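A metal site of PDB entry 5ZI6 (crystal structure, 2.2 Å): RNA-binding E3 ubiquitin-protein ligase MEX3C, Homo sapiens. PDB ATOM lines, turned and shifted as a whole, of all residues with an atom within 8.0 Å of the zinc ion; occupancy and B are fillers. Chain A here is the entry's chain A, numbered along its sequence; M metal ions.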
ATOM      1  N   ASP A   3      -5.324   3.637   7.577  1.00  0.00           N
ATOM      2  CA  ASP A   3      -6.699   3.191   7.811  1.00  0.00           C
ATOM      3  C   ASP A   3      -7.024   3.231   9.297  1.00  0.00           C
ATOM      4  O   ASP A   3      -6.261   2.693  10.113  1.00  0.00           O
ATOM      5  CB  ASP A   3      -6.900   1.761   7.286  1.00  0.00           C
ATOM      6  CG  ASP A   3      -7.269   1.715   5.792  1.00  0.00           C
ATOM      7  OD1 ASP A   3      -7.596   2.781   5.229  1.00  0.00           O
ATOM      8  OD2 ASP A   3      -7.253   0.606   5.206  1.00  0.00           O
ATOM      9  N   CYS A   4      -8.140   3.882   9.642  1.00  0.00           N
ATOM     10  CA  CYS A   4      -8.702   3.895  10.998  1.00  0.00           C
ATOM     11  C   CYS A   4      -8.619   2.526  11.643  1.00  0.00           C
ATOM     12  O   CYS A   4      -9.021   1.529  11.048  1.00  0.00           O
ATOM     13  CB  CYS A   4     -10.155   4.341  10.956  1.00  0.00           C
ATOM     14  SG  CYS A   4     -11.048   4.094  12.544  1.00  0.00           S
ATOM     15  N   VAL A   5      -8.074   2.469  12.863  1.00  0.00           N
ATOM     16  CA  VAL A   5      -7.880   1.192  13.545  1.00  0.00           C
ATOM     17  C   VAL A   5      -9.155   0.624  14.152  1.00  0.00           C
ATOM     18  O   VAL A   5      -9.140  -0.524  14.617  1.00  0.00           O
ATOM     19  CB  VAL A   5      -6.820   1.280  14.664  1.00  0.00           C
ATOM     20  CG1 VAL A   5      -5.527   1.846  14.126  1.00  0.00           C
ATOM     21  CG2 VAL A   5      -7.327   2.143  15.810  1.00  0.00           C
ATOM     22  N   ILE A   6     -10.269   1.361  14.119  1.00  0.00           N
ATOM     23  CA  ILE A   6     -11.531   0.855  14.675  1.00  0.00           C
ATOM     24  C   ILE A   6     -12.328   0.175  13.555  1.00  0.00           C
ATOM     25  O   ILE A   6     -12.726  -0.984  13.687  1.00  0.00           O
ATOM     26  CB  ILE A   6     -12.344   1.965  15.374  1.00  0.00           C
ATOM     27  CG1 ILE A   6     -11.564   2.553  16.548  1.00  0.00           C
ATOM     28  CG2 ILE A   6     -13.652   1.401  15.956  1.00  0.00           C
ATOM     29  CD1 ILE A   6     -11.020   1.525  17.511  1.00  0.00           C
ATOM     30  N   CYS A   7     -12.581   0.903  12.462  1.00  0.00           N
ATOM     31  CA  CYS A   7     -13.379   0.358  11.365  1.00  0.00           C
ATOM     32  C   CYS A   7     -12.567  -0.218  10.197  1.00  0.00           C
ATOM     33  O   CYS A   7     -13.088  -1.059   9.460  1.00  0.00           O
ATOM     34  CB  CYS A   7     -14.335   1.418  10.820  1.00  0.00           C
ATOM     35  SG  CYS A   7     -13.493   2.846  10.101  1.00  0.00           S
ATOM     36  N   PHE A   8     -11.311   0.209  10.012  1.00  0.00           N
ATOM     37  CA  PHE A   8     -10.523  -0.191   8.831  1.00  0.00           C
ATOM     38  C   PHE A   8     -11.265   0.100   7.523  1.00  0.00           C
ATOM     39  O   PHE A   8     -11.204  -0.689   6.572  1.00  0.00           O
ATOM     40  CB  PHE A   8     -10.112  -1.646   8.916  1.00  0.00           C
ATOM     41  CG  PHE A   8      -9.186  -1.958  10.054  1.00  0.00           C
ATOM     42  CD1 PHE A   8      -7.831  -1.693   9.936  1.00  0.00           C
ATOM     43  CD2 PHE A   8      -9.664  -2.501  11.231  1.00  0.00           C
ATOM     44  CE1 PHE A   8      -6.967  -1.978  10.962  1.00  0.00           C
ATOM     45  CE2 PHE A   8      -8.799  -2.788  12.287  1.00  0.00           C
ATOM     46  CZ  PHE A   8      -7.442  -2.529  12.145  1.00  0.00           C
ATOM     47  N   GLU A   9     -11.954   1.206   7.472  1.00  0.00           N
ATOM     48  CA  GLU A   9     -12.750   1.574   6.302  1.00  0.00           C
ATOM     49  C   GLU A   9     -12.494   3.002   5.861  1.00  0.00           C
ATOM     50  O   GLU A   9     -12.496   3.264   4.656  1.00  0.00           O
ATOM     51  CB  GLU A   9     -14.258   1.415   6.569  1.00  0.00           C
ATOM     52  CG  GLU A   9     -14.801  -0.003   6.594  1.00  0.00           C
ATOM     53  CD  GLU A   9     -16.322  -0.002   6.658  1.00  0.00           C
ATOM     54  OE1 GLU A   9     -16.918   1.089   6.484  1.00  0.00           O
ATOM     55  OE2 GLU A   9     -16.936  -1.062   6.889  1.00  0.00           O
ATOM     56  N   ASN A  10     -12.301   3.921   6.789  1.00  0.00           N
ATOM     57  CA  ASN A  10     -12.048   5.314   6.456  1.00  0.00           C
ATOM     58  C   ASN A  10     -10.608   5.652   6.778  1.00  0.00           C
ATOM     59  O   ASN A  10      -9.936   4.953   7.548  1.00  0.00           O
ATOM     60  CB  ASN A  10     -12.980   6.246   7.221  1.00  0.00           C
ATOM     61  CG  ASN A  10     -14.434   5.898   7.043  1.00  0.00           C
ATOM     62  OD1 ASN A  10     -14.818   5.292   6.048  1.00  0.00           O
ATOM     63  ND2 ASN A  10     -15.266   6.289   8.013  1.00  0.00           N
ATOM     64  N   GLU A  11     -10.134   6.748   6.199  1.00  0.00           N
ATOM     65  CA  GLU A  11      -8.793   7.247   6.454  1.00  0.00           C
ATOM     66  C   GLU A  11      -8.655   7.795   7.860  1.00  0.00           C
ATOM     67  O   GLU A  11      -9.635   8.235   8.470  1.00  0.00           O
ATOM     68  CB  GLU A  11      -8.436   8.356   5.473  1.00  0.00           C
ATOM     69  CG  GLU A  11      -7.706   7.854   4.323  1.00  0.00           C
ATOM     70  CD  GLU A  11      -8.270   8.453   3.063  1.00  0.00           C
ATOM     71  OE1 GLU A  11      -8.169   7.776   2.018  1.00  0.00           O
ATOM     72  OE2 GLU A  11      -8.803   9.583   3.107  1.00  0.00           O
ATOM     73  N   VAL A  12      -7.420   7.778   8.361  1.00  0.00           N
ATOM     74  CA  VAL A  12      -7.110   8.401   9.632  1.00  0.00           C
ATOM     75  C   VAL A  12      -7.173   9.905   9.455  1.00  0.00           C
ATOM     76  O   VAL A  12      -6.521  10.485   8.573  1.00  0.00           O
ATOM     77  CB  VAL A  12      -5.733   7.933  10.136  1.00  0.00           C
ATOM     78  CG1 VAL A  12      -5.257   8.769  11.337  1.00  0.00           C
ATOM     79  CG2 VAL A  12      -5.798   6.449  10.513  1.00  0.00           C
ATOM     80  N   LEU A  23      -5.199   7.711  15.098  1.00  0.00           N
ATOM     81  CA  LEU A  23      -5.447   6.409  14.485  1.00  0.00           C
ATOM     82  C   LEU A  23      -6.919   6.227  14.100  1.00  0.00           C
ATOM     83  O   LEU A  23      -7.374   5.082  13.972  1.00  0.00           O
ATOM     84  CB  LEU A  23      -5.042   5.288  15.446  1.00  0.00           C
ATOM     85  CG  LEU A  23      -3.552   5.248  15.763  1.00  0.00           C
ATOM     86  CD1 LEU A  23      -3.242   4.302  16.932  1.00  0.00           C
ATOM     87  CD2 LEU A  23      -2.818   4.823  14.520  1.00  0.00           C
ATOM     88  N   PHE A  24      -7.668   7.308  13.974  1.00  0.00           N
ATOM     89  CA  PHE A  24      -9.116   7.192  13.878  1.00  0.00           C
ATOM     90  C   PHE A  24      -9.634   8.063  12.735  1.00  0.00           C
ATOM     91  O   PHE A  24      -9.088   9.138  12.449  1.00  0.00           O
ATOM     92  CB  PHE A  24      -9.773   7.601  15.219  1.00  0.00           C
ATOM     93  CG  PHE A  24      -9.126   6.973  16.429  1.00  0.00           C
ATOM     94  CD1 PHE A  24      -9.383   5.658  16.756  1.00  0.00           C
ATOM     95  CD2 PHE A  24      -8.218   7.696  17.204  1.00  0.00           C
ATOM     96  CE1 PHE A  24      -8.752   5.056  17.858  1.00  0.00           C
ATOM     97  CE2 PHE A  24      -7.589   7.107  18.306  1.00  0.00           C
ATOM     98  CZ  PHE A  24      -7.867   5.782  18.634  1.00  0.00           C
ATOM     99  N   CYS A  25     -10.674   7.572  12.077  1.00  0.00           N
ATOM    100  CA  CYS A  25     -11.496   8.446  11.254  1.00  0.00           C
ATOM    101  C   CYS A  25     -12.304   9.336  12.190  1.00  0.00           C
ATOM    102  O   CYS A  25     -12.353   9.124  13.399  1.00  0.00           O
ATOM    103  CB  CYS A  25     -12.384   7.614  10.326  1.00  0.00           C
ATOM    104  SG  CYS A  25     -13.729   6.570  11.071  1.00  0.00           S
ATOM    105  N   MET A  26     -12.904  10.384  11.625  1.00  0.00           N
ATOM    106  CA  MET A  26     -13.631  11.296  12.504  1.00  0.00           C
ATOM    107  C   MET A  26     -14.911  10.646  13.036  1.00  0.00           C
ATOM    108  O   MET A  26     -15.322  10.938  14.159  1.00  0.00           O
ATOM    109  CB  MET A  26     -13.934  12.610  11.783  1.00  0.00           C
ATOM    110  CG  MET A  26     -14.273  13.773  12.743  1.00  0.00           C
ATOM    111  SD  MET A  26     -12.913  14.403  13.773  1.00  0.00           S
ATOM    112  CE  MET A  26     -13.763  15.102  15.186  1.00  0.00           C
ATOM    113  N   GLU A  27     -15.571   9.788  12.250  1.00  0.00           N
ATOM    114  CA  GLU A  27     -16.777   9.148  12.782  1.00  0.00           C
ATOM    115  C   GLU A  27     -16.441   8.250  13.955  1.00  0.00           C
ATOM    116  O   GLU A  27     -17.136   8.285  14.976  1.00  0.00           O
ATOM    117  CB  GLU A  27     -17.540   8.364  11.702  1.00  0.00           C
ATOM    118  CG  GLU A  27     -18.150   9.201  10.559  1.00  0.00           C
ATOM    119  CD  GLU A  27     -17.249   9.399   9.336  1.00  0.00           C
ATOM    120  OE1 GLU A  27     -16.029   9.112   9.407  1.00  0.00           O
ATOM    121  OE2 GLU A  27     -17.765   9.899   8.309  1.00  0.00           O
ATOM    122  N   CYS A  28     -15.391   7.433  13.854  1.00  0.00           N
ATOM    123  CA  CYS A  28     -15.050   6.559  14.971  1.00  0.00           C
ATOM    124  C   CYS A  28     -14.584   7.358  16.184  1.00  0.00           C
ATOM    125  O   CYS A  28     -14.962   7.038  17.326  1.00  0.00           O
ATOM    126  CB  CYS A  28     -14.011   5.538  14.530  1.00  0.00           C
ATOM    127  SG  CYS A  28     -14.705   4.344  13.398  1.00  0.00           S
ATOM    128  N   ALA A  29     -13.822   8.424  15.968  1.00  0.00           N
ATOM    129  CA  ALA A  29     -13.407   9.264  17.079  1.00  0.00           C
ATOM    130  C   ALA A  29     -14.593   9.957  17.745  1.00  0.00           C
ATOM    131  O   ALA A  29     -14.645  10.073  18.971  1.00  0.00           O
ATOM    132  CB  ALA A  29     -12.372  10.297  16.610  1.00  0.00           C
ATOM    133  N   LYS A  31     -17.600   8.784  17.854  1.00  0.00           N
ATOM    134  CA  LYS A  31     -18.282   7.761  18.643  1.00  0.00           C
ATOM    135  C   LYS A  31     -17.556   7.532  19.965  1.00  0.00           C
ATOM    136  O   LYS A  31     -18.191   7.268  20.984  1.00  0.00           O
ATOM    137  CB  LYS A  31     -18.370   6.455  17.863  1.00  0.00           C
ATOM    138  CG  LYS A  31     -19.542   6.371  16.899  1.00  0.00           C
ATOM    139  CD  LYS A  31     -19.356   5.232  15.896  1.00  0.00           C
ATOM    140  CE  LYS A  31     -20.150   5.470  14.626  1.00  0.00           C
ATOM    141  NZ  LYS A  31     -19.897   4.458  13.548  1.00  0.00           N
HETATM  142 ZN    ZN M   1     -13.213   4.564  11.658  1.00  0.00          ZN
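SG of Cys 25 binds the zinc ion (2.2 Å). The zinc ion is bound by SG of Cys 28, at 2.3 Å. The zinc ion is bound by SG of Cys 7, at 2.3 Å. SG of Cys 4 binds the zinc ion, at 2.4 Å. The zinc ion has four donor atoms within binding distance.
The side-chain amide nitrogen of Asn 10 lies close to the side-chain sulfur of Cys 25. SG of Cys 7 sits close to N of Asn 10 (3.7 Å). The side-chain sulfur (SG) of Cys 7 sits close to the backbone NH (N) of Glu 9, at 3.5 Å. The backbone carbonyl oxygen (O) of Asn 10 sits at hydrogen-bond distance from the backbone NH (N) of Cys 4 (3.0 Å). The side-chain sulfur (SG) of Cys 4 sits close to the backbone NH (N) of Ile 6, at 3.2 Å.
Within 4 Å of the zinc ion: Cys 4, Cys 7, Cys 25 and Cys 28. The nearest printed residue that does not touch the zinc ion is Asn 10 (4.5 Å).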
